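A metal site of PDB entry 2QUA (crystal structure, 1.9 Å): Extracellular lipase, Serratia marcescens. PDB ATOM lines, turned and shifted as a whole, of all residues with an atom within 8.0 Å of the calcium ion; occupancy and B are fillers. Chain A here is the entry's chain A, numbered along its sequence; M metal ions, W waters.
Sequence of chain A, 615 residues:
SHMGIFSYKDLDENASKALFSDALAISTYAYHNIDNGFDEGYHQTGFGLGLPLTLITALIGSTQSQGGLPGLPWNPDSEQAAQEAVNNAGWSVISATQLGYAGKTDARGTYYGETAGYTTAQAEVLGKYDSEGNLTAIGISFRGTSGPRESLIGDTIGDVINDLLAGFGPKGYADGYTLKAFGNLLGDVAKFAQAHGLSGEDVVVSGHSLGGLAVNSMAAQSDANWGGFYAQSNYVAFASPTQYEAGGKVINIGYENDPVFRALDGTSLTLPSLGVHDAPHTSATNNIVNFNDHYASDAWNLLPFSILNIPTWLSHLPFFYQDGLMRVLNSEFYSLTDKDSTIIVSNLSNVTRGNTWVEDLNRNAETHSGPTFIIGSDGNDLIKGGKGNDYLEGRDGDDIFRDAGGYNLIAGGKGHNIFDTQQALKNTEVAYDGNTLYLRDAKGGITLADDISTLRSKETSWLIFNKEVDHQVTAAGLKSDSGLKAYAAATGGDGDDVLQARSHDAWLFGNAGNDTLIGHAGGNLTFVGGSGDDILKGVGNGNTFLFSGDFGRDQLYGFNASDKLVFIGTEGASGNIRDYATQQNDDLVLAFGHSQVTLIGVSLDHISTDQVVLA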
ATOM      1  N   TYR A 255     -13.800  21.353 -19.273  1.00  0.00           N
ATOM      2  CA  TYR A 255     -12.426  20.909 -19.487  1.00  0.00           C
ATOM      3  C   TYR A 255     -12.414  19.480 -20.052  1.00  0.00           C
ATOM      4  O   TYR A 255     -13.191  18.636 -19.596  1.00  0.00           O
ATOM      5  CB  TYR A 255     -11.677  20.879 -18.180  1.00  0.00           C
ATOM      6  CG  TYR A 255     -11.412  22.211 -17.508  1.00  0.00           C
ATOM      7  CD1 TYR A 255     -10.495  23.123 -18.046  1.00  0.00           C
ATOM      8  CD2 TYR A 255     -12.079  22.544 -16.330  1.00  0.00           C
ATOM      9  CE1 TYR A 255     -10.231  24.333 -17.412  1.00  0.00           C
ATOM     10  CE2 TYR A 255     -11.833  23.765 -15.685  1.00  0.00           C
ATOM     11  CZ  TYR A 255     -10.900  24.647 -16.245  1.00  0.00           C
ATOM     12  OH  TYR A 255     -10.644  25.842 -15.610  1.00  0.00           O
ATOM     13  N   GLU A 256     -11.539  19.210 -21.031  1.00  0.00           N
ATOM     14  CA  GLU A 256     -11.507  17.894 -21.676  1.00  0.00           C
ATOM     15  C   GLU A 256     -11.078  16.789 -20.701  1.00  0.00           C
ATOM     16  O   GLU A 256     -11.477  15.644 -20.854  1.00  0.00           O
ATOM     17  CB  GLU A 256     -10.626  17.890 -22.953  1.00  0.00           C
ATOM     18  CG  GLU A 256      -9.153  17.996 -22.703  1.00  0.00           C
ATOM     19  CD  GLU A 256      -8.330  17.942 -23.998  1.00  0.00           C
ATOM     20  OE1 GLU A 256      -8.906  18.013 -25.115  1.00  0.00           O
ATOM     21  OE2 GLU A 256      -7.080  17.840 -23.909  1.00  0.00           O
ATOM     22  N   ASN A 257     -10.277  17.127 -19.682  1.00  0.00           N
ATOM     23  CA  ASN A 257      -9.893  16.119 -18.697  1.00  0.00           C
ATOM     24  C   ASN A 257     -10.869  16.066 -17.509  1.00  0.00           C
ATOM     25  O   ASN A 257     -10.595  15.395 -16.498  1.00  0.00           O
ATOM     26  CB  ASN A 257      -8.448  16.296 -18.238  1.00  0.00           C
ATOM     27  CG  ASN A 257      -8.173  17.692 -17.658  1.00  0.00           C
ATOM     28  OD1 ASN A 257      -8.623  18.698 -18.206  1.00  0.00           O
ATOM     29  ND2 ASN A 257      -7.415  17.738 -16.571  1.00  0.00           N
ATOM     30  N   PHE A 261     -17.715  16.043 -18.076  1.00  0.00           N
ATOM     31  CA  PHE A 261     -17.960  16.828 -19.278  1.00  0.00           C
ATOM     32  C   PHE A 261     -18.066  15.913 -20.519  1.00  0.00           C
ATOM     33  O   PHE A 261     -17.082  15.277 -20.904  1.00  0.00           O
ATOM     34  CB  PHE A 261     -16.819  17.862 -19.418  1.00  0.00           C
ATOM     35  CG  PHE A 261     -16.991  18.816 -20.581  1.00  0.00           C
ATOM     36  CD1 PHE A 261     -18.185  19.521 -20.770  1.00  0.00           C
ATOM     37  CD2 PHE A 261     -15.952  19.020 -21.473  1.00  0.00           C
ATOM     38  CE1 PHE A 261     -18.330  20.406 -21.838  1.00  0.00           C
ATOM     39  CE2 PHE A 261     -16.086  19.910 -22.562  1.00  0.00           C
ATOM     40  CZ  PHE A 261     -17.277  20.607 -22.747  1.00  0.00           C
ATOM     41  N   ARG A 262     -19.258  15.867 -21.127  1.00  0.00           N
ATOM     42  CA  ARG A 262     -19.518  15.084 -22.339  1.00  0.00           C
ATOM     43  C   ARG A 262     -19.494  13.576 -22.082  1.00  0.00           C
ATOM     44  O   ARG A 262     -19.292  12.821 -23.013  1.00  0.00           O
ATOM     45  CB  ARG A 262     -18.507  15.415 -23.463  1.00  0.00           C
ATOM     46  CG  ARG A 262     -18.415  16.885 -23.857  1.00  0.00           C
ATOM     47  CD  ARG A 262     -17.132  17.188 -24.646  1.00  0.00           C
ATOM     48  NE  ARG A 262     -15.957  16.676 -23.935  1.00  0.00           N
ATOM     49  CZ  ARG A 262     -14.740  16.568 -24.475  1.00  0.00           C
ATOM     50  NH1 ARG A 262     -14.543  16.950 -25.719  1.00  0.00           N
ATOM     51  NH2 ARG A 262     -13.721  16.079 -23.771  1.00  0.00           N
ATOM     52  N   HIS A 277     -13.729  10.134 -23.241  1.00  0.00           N
ATOM     53  CA  HIS A 277     -14.770  10.491 -24.178  1.00  0.00           C
ATOM     54  C   HIS A 277     -14.541  11.901 -24.700  1.00  0.00           C
ATOM     55  O   HIS A 277     -15.270  12.838 -24.344  1.00  0.00           O
ATOM     56  CB  HIS A 277     -16.157  10.354 -23.514  1.00  0.00           C
ATOM     57  CG  HIS A 277     -16.188  10.860 -22.117  1.00  0.00           C
ATOM     58  ND1 HIS A 277     -16.214  10.030 -21.010  1.00  0.00           N
ATOM     59  CD2 HIS A 277     -16.182  12.125 -21.633  1.00  0.00           C
ATOM     60  CE1 HIS A 277     -16.231  10.758 -19.908  1.00  0.00           C
ATOM     61  NE2 HIS A 277     -16.209  12.035 -20.258  1.00  0.00           N
ATOM     62  N   ASP A 278     -13.515  12.037 -25.549  1.00  0.00           N
ATOM     63  CA  ASP A 278     -13.081  13.335 -26.042  1.00  0.00           C
ATOM     64  C   ASP A 278     -13.456  13.497 -27.508  1.00  0.00           C
ATOM     65  O   ASP A 278     -12.859  14.318 -28.205  1.00  0.00           O
ATOM     66  CB  ASP A 278     -11.562  13.545 -25.823  1.00  0.00           C
ATOM     67  CG  ASP A 278     -11.074  14.977 -26.150  1.00  0.00           C
ATOM     68  OD1 ASP A 278     -11.783  15.966 -25.828  1.00  0.00           O
ATOM     69  OD2 ASP A 278      -9.963  15.139 -26.722  1.00  0.00           O
ATOM     70  N   ALA A 279     -14.417  12.710 -28.013  1.00  0.00           N
ATOM     71  CA  ALA A 279     -14.852  12.939 -29.400  1.00  0.00           C
ATOM     72  C   ALA A 279     -15.483  14.315 -29.418  1.00  0.00           C
ATOM     73  O   ALA A 279     -16.221  14.664 -28.502  1.00  0.00           O
ATOM     74  CB  ALA A 279     -15.814  11.863 -29.908  1.00  0.00           C
ATOM     75  N   PRO A 280     -15.179  15.125 -30.438  1.00  0.00           N
ATOM     76  CA  PRO A 280     -15.633  16.504 -30.357  1.00  0.00           C
ATOM     77  C   PRO A 280     -17.114  16.668 -30.692  1.00  0.00           C
ATOM     78  O   PRO A 280     -17.602  16.105 -31.664  1.00  0.00           O
ATOM     79  CB  PRO A 280     -14.734  17.228 -31.379  1.00  0.00           C
ATOM     80  CG  PRO A 280     -14.322  16.160 -32.354  1.00  0.00           C
ATOM     81  CD  PRO A 280     -14.409  14.837 -31.665  1.00  0.00           C
ATOM     82  N   THR A 285     -16.862  23.215 -26.216  1.00  0.00           N
ATOM     83  CA  THR A 285     -15.457  23.602 -26.246  1.00  0.00           C
ATOM     84  C   THR A 285     -14.652  22.327 -26.018  1.00  0.00           C
ATOM     85  O   THR A 285     -14.553  21.840 -24.893  1.00  0.00           O
ATOM     86  CB  THR A 285     -15.143  24.621 -25.143  1.00  0.00           C
ATOM     87  OG1 THR A 285     -15.545  24.094 -23.877  1.00  0.00           O
ATOM     88  CG2 THR A 285     -15.892  25.924 -25.387  1.00  0.00           C
ATOM     89  N   ASN A 286     -14.081  21.755 -27.081  1.00  0.00           N
ATOM     90  CA  ASN A 286     -13.563  20.392 -26.948  1.00  0.00           C
ATOM     91  C   ASN A 286     -12.138  20.229 -26.459  1.00  0.00           C
ATOM     92  O   ASN A 286     -11.697  19.100 -26.183  1.00  0.00           O
ATOM     93  CB  ASN A 286     -13.754  19.665 -28.271  1.00  0.00           C
ATOM     94  CG  ASN A 286     -15.209  19.380 -28.563  1.00  0.00           C
ATOM     95  OD1 ASN A 286     -15.876  18.683 -27.788  1.00  0.00           O
ATOM     96  ND2 ASN A 286     -15.712  19.920 -29.659  1.00  0.00           N
ATOM     97  N   ASN A 287     -11.413  21.341 -26.345  1.00  0.00           N
ATOM     98  CA  ASN A 287      -9.961  21.242 -26.154  1.00  0.00           C
ATOM     99  C   ASN A 287      -9.360  22.169 -25.097  1.00  0.00           C
ATOM    100  O   ASN A 287      -8.260  22.702 -25.273  1.00  0.00           O
ATOM    101  CB  ASN A 287      -9.265  21.432 -27.506  1.00  0.00           C
ATOM    102  CG  ASN A 287      -9.756  20.456 -28.544  1.00  0.00           C
ATOM    103  OD1 ASN A 287      -9.665  19.240 -28.351  1.00  0.00           O
ATOM    104  ND2 ASN A 287     -10.286  20.975 -29.653  1.00  0.00           N
ATOM    105  N   ILE A 288     -10.096  22.371 -24.003  1.00  0.00           N
ATOM    106  CA  ILE A 288      -9.585  23.144 -22.883  1.00  0.00           C
ATOM    107  C   ILE A 288      -9.093  22.190 -21.783  1.00  0.00           C
ATOM    108  O   ILE A 288      -9.850  21.352 -21.288  1.00  0.00           O
ATOM    109  CB  ILE A 288     -10.646  24.058 -22.256  1.00  0.00           C
ATOM    110  CG1 ILE A 288     -11.350  24.899 -23.315  1.00  0.00           C
ATOM    111  CG2 ILE A 288      -9.984  24.949 -21.181  1.00  0.00           C
ATOM    112  CD1 ILE A 288     -12.489  25.773 -22.718  1.00  0.00           C
ATOM    113  N   VAL A 289      -7.820  22.342 -21.422  1.00  0.00           N
ATOM    114  CA  VAL A 289      -7.197  21.514 -20.405  1.00  0.00           C
ATOM    115  C   VAL A 289      -7.123  22.217 -19.030  1.00  0.00           C
ATOM    116  O   VAL A 289      -6.661  23.376 -18.925  1.00  0.00           O
ATOM    117  CB  VAL A 289      -5.806  21.056 -20.894  1.00  0.00           C
ATOM    118  CG1 VAL A 289      -5.086  20.246 -19.837  1.00  0.00           C
ATOM    119  CG2 VAL A 289      -5.950  20.265 -22.213  1.00  0.00           C
ATOM    120  N   ASP A 340     -13.009  25.602 -30.507  1.00  0.00           N
ATOM    121  CA  ASP A 340     -12.159  24.415 -30.338  1.00  0.00           C
ATOM    122  C   ASP A 340     -10.654  24.716 -30.250  1.00  0.00           C
ATOM    123  O   ASP A 340      -9.843  23.830 -30.454  1.00  0.00           O
ATOM    124  CB  ASP A 340     -12.479  23.384 -31.456  1.00  0.00           C
ATOM    125  CG  ASP A 340     -13.839  22.705 -31.235  1.00  0.00           C
ATOM    126  OD1 ASP A 340     -14.185  22.481 -30.052  1.00  0.00           O
ATOM    127  OD2 ASP A 340     -14.561  22.397 -32.202  1.00  0.00           O
ATOM    128  N   SER A 341     -10.280  25.953 -29.919  1.00  0.00           N
ATOM    129  CA  SER A 341      -8.863  26.226 -29.615  1.00  0.00           C
ATOM    130  C   SER A 341      -8.282  25.305 -28.510  1.00  0.00           C
ATOM    131  O   SER A 341      -8.955  25.019 -27.492  1.00  0.00           O
ATOM    132  CB  SER A 341      -8.634  27.702 -29.249  1.00  0.00           C
ATOM    133  OG  SER A 341      -9.002  28.572 -30.334  1.00  0.00           O
ATOM    134  N   THR A 342      -7.048  24.838 -28.716  1.00  0.00           N
ATOM    135  CA  THR A 342      -6.350  24.166 -27.638  1.00  0.00           C
ATOM    136  C   THR A 342      -5.907  25.203 -26.587  1.00  0.00           C
ATOM    137  O   THR A 342      -5.030  26.055 -26.852  1.00  0.00           O
ATOM    138  CB  THR A 342      -5.091  23.444 -28.135  1.00  0.00           C
ATOM    139  OG1 THR A 342      -5.397  22.620 -29.272  1.00  0.00           O
ATOM    140  CG2 THR A 342      -4.483  22.603 -26.997  1.00  0.00           C
ATOM    141  N   ASN A 362      -1.211  16.654 -23.702  1.00  0.00           N
ATOM    142  CA  ASN A 362      -2.220  15.984 -24.567  1.00  0.00           C
ATOM    143  C   ASN A 362      -2.723  14.675 -23.972  1.00  0.00           C
ATOM    144  O   ASN A 362      -3.082  13.723 -24.685  1.00  0.00           O
ATOM    145  CB  ASN A 362      -1.639  15.731 -25.969  1.00  0.00           C
ATOM    146  CG  ASN A 362      -2.692  15.792 -27.085  1.00  0.00           C
ATOM    147  OD1 ASN A 362      -2.467  16.424 -28.135  1.00  0.00           O
ATOM    148  ND2 ASN A 362      -3.846  15.141 -26.875  1.00  0.00           N
ATOM    149  N   ARG A 363      -2.782  14.630 -22.644  1.00  0.00           N
ATOM    150  CA  ARG A 363      -3.087  13.410 -21.946  1.00  0.00           C
ATOM    151  C   ARG A 363      -4.581  13.066 -22.072  1.00  0.00           C
ATOM    152  O   ARG A 363      -5.438  13.956 -21.997  1.00  0.00           O
ATOM    153  CB  ARG A 363      -2.688  13.566 -20.468  1.00  0.00           C
ATOM    154  CG  ARG A 363      -2.087  12.316 -19.860  1.00  0.00           C
ATOM    155  CD  ARG A 363      -2.024  12.397 -18.348  1.00  0.00           C
ATOM    156  NE  ARG A 363      -0.922  13.165 -17.754  1.00  0.00           N
ATOM    157  CZ  ARG A 363       0.322  12.703 -17.571  1.00  0.00           C
ATOM    158  NH1 ARG A 363       0.642  11.478 -17.967  1.00  0.00           N
ATOM    159  NH2 ARG A 363       1.241  13.473 -16.998  1.00  0.00           N
ATOM    160  N   ASN A 364      -4.886  11.782 -22.263  1.00  0.00           N
ATOM    161  CA  ASN A 364      -6.289  11.324 -22.272  1.00  0.00           C
ATOM    162  C   ASN A 364      -7.198  12.232 -23.115  1.00  0.00           C
ATOM    163  O   ASN A 364      -8.209  12.757 -22.620  1.00  0.00           O
ATOM    164  CB  ASN A 364      -6.826  11.254 -20.840  1.00  0.00           C
ATOM    165  CG  ASN A 364      -6.078  10.252 -19.965  1.00  0.00           C
ATOM    166  OD1 ASN A 364      -5.591  10.587 -18.871  1.00  0.00           O
ATOM    167  ND2 ASN A 364      -5.979   9.018 -20.436  1.00  0.00           N
ATOM    168  N   ALA A 365      -6.821  12.424 -24.379  1.00  0.00           N
ATOM    169  CA  ALA A 365      -7.552  13.337 -25.272  1.00  0.00           C
ATOM    170  C   ALA A 365      -7.122  13.114 -26.715  1.00  0.00           C
ATOM    171  O   ALA A 365      -6.010  12.659 -26.974  1.00  0.00           O
ATOM    172  CB  ALA A 365      -7.291  14.765 -24.882  1.00  0.00           C
ATOM    173  N   GLU A 366      -8.004  13.424 -27.667  1.00  0.00           N
ATOM    174  CA  GLU A 366      -7.632  13.366 -29.081  1.00  0.00           C
ATOM    175  C   GLU A 366      -6.413  14.259 -29.291  1.00  0.00           C
ATOM    176  O   GLU A 366      -6.201  15.220 -28.551  1.00  0.00           O
ATOM    177  CB  GLU A 366      -8.786  13.826 -29.985  1.00  0.00           C
ATOM    178  CG  GLU A 366     -10.086  13.051 -29.808  1.00  0.00           C
ATOM    179  CD  GLU A 366     -11.063  13.257 -30.972  1.00  0.00           C
ATOM    180  OE1 GLU A 366     -10.842  14.167 -31.836  1.00  0.00           O
ATOM    181  OE2 GLU A 366     -12.055  12.517 -31.024  1.00  0.00           O
ATOM    182  N   THR A 367      -5.622  13.950 -30.311  1.00  0.00           N
ATOM    183  CA  THR A 367      -4.490  14.786 -30.680  1.00  0.00           C
ATOM    184  C   THR A 367      -4.924  16.230 -30.934  1.00  0.00           C
ATOM    185  O   THR A 367      -5.844  16.484 -31.737  1.00  0.00           O
ATOM    186  CB  THR A 367      -3.810  14.251 -31.959  1.00  0.00           C
ATOM    187  OG1 THR A 367      -3.538  12.863 -31.801  1.00  0.00           O
ATOM    188  CG2 THR A 367      -2.514  15.018 -32.235  1.00  0.00           C
ATOM    189  N   HIS A 368      -4.276  17.168 -30.261  1.00  0.00           N
ATOM    190  CA  HIS A 368      -4.566  18.582 -30.446  1.00  0.00           C
ATOM    191  C   HIS A 368      -3.964  19.077 -31.754  1.00  0.00           C
ATOM    192  O   HIS A 368      -2.952  18.540 -32.227  1.00  0.00           O
ATOM    193  CB  HIS A 368      -3.975  19.401 -29.288  1.00  0.00           C
ATOM    194  CG  HIS A 368      -4.548  19.066 -27.941  1.00  0.00           C
ATOM    195  ND1 HIS A 368      -3.775  19.064 -26.798  1.00  0.00           N
ATOM    196  CD2 HIS A 368      -5.800  18.728 -27.562  1.00  0.00           C
ATOM    197  CE1 HIS A 368      -4.536  18.735 -25.764  1.00  0.00           C
ATOM    198  NE2 HIS A 368      -5.773  18.529 -26.204  1.00  0.00           N
HETATM  199 CA    CA M   1     -10.225  17.450 -26.969  1.00  0.00          CA
HETATM  200  O   HOH W   1      -8.414  16.966 -28.425  1.00  0.00           O
HETATM  201  O   HOH W   2     -11.762  16.763 -28.626  1.00  0.00           O
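Of the 24 residues printed, 4 come within 4 Å of the calcium ion. Along chain A the residues within 4 Å of the calcium ion span positions 256 to 287. The nearest printed residue that does not touch the calcium ion is Ala 365 (4.5 Å).
ND2 of Asn 287 lies within hydrogen-bond range of O of Asp 340, at 3.0 Å. OD1 of Asp 278 lies close to NH2 of Arg 262, at 2.8 Å. OD2 of Asp 278 sits close to N of Glu 366, at 2.8 Å. The side-chain carboxylate (OE2) of Glu 256 sits at hydrogen-bond distance from a ring nitrogen (NE2) of His 368 (2.7 Å). The backbone NH (N) of Glu 256 is in hydrogen-bond range of the backbone carbonyl oxygen (O) of Ile 288 (2.7 Å). The side-chain amide oxygen (OD1) of Asn 286 lies within hydrogen-bond range of the guanidinium group (NH1) of Arg 262 (3.0 Å). The side-chain carboxylate of Asp 340 is in hydrogen-bond range of the side-chain amide nitrogen of Asn 286 (3.0 Å).
The calcium ion is bound by the side-chain amide oxygen (OD1) of Asn 287 (2.3 Å), the side-chain carboxylate (OD2) of Asp 278 (2.3 Å), the side-chain carboxylate (OE1) of Glu 256 (2.3 Å), the backbone carbonyl oxygen (O) of Asn 286 (2.3 Å), water W2 (2.4 Å), water W1 (2.4 Å) and the side-chain carboxylate (OD1) of Asp 278 (2.4 Å).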
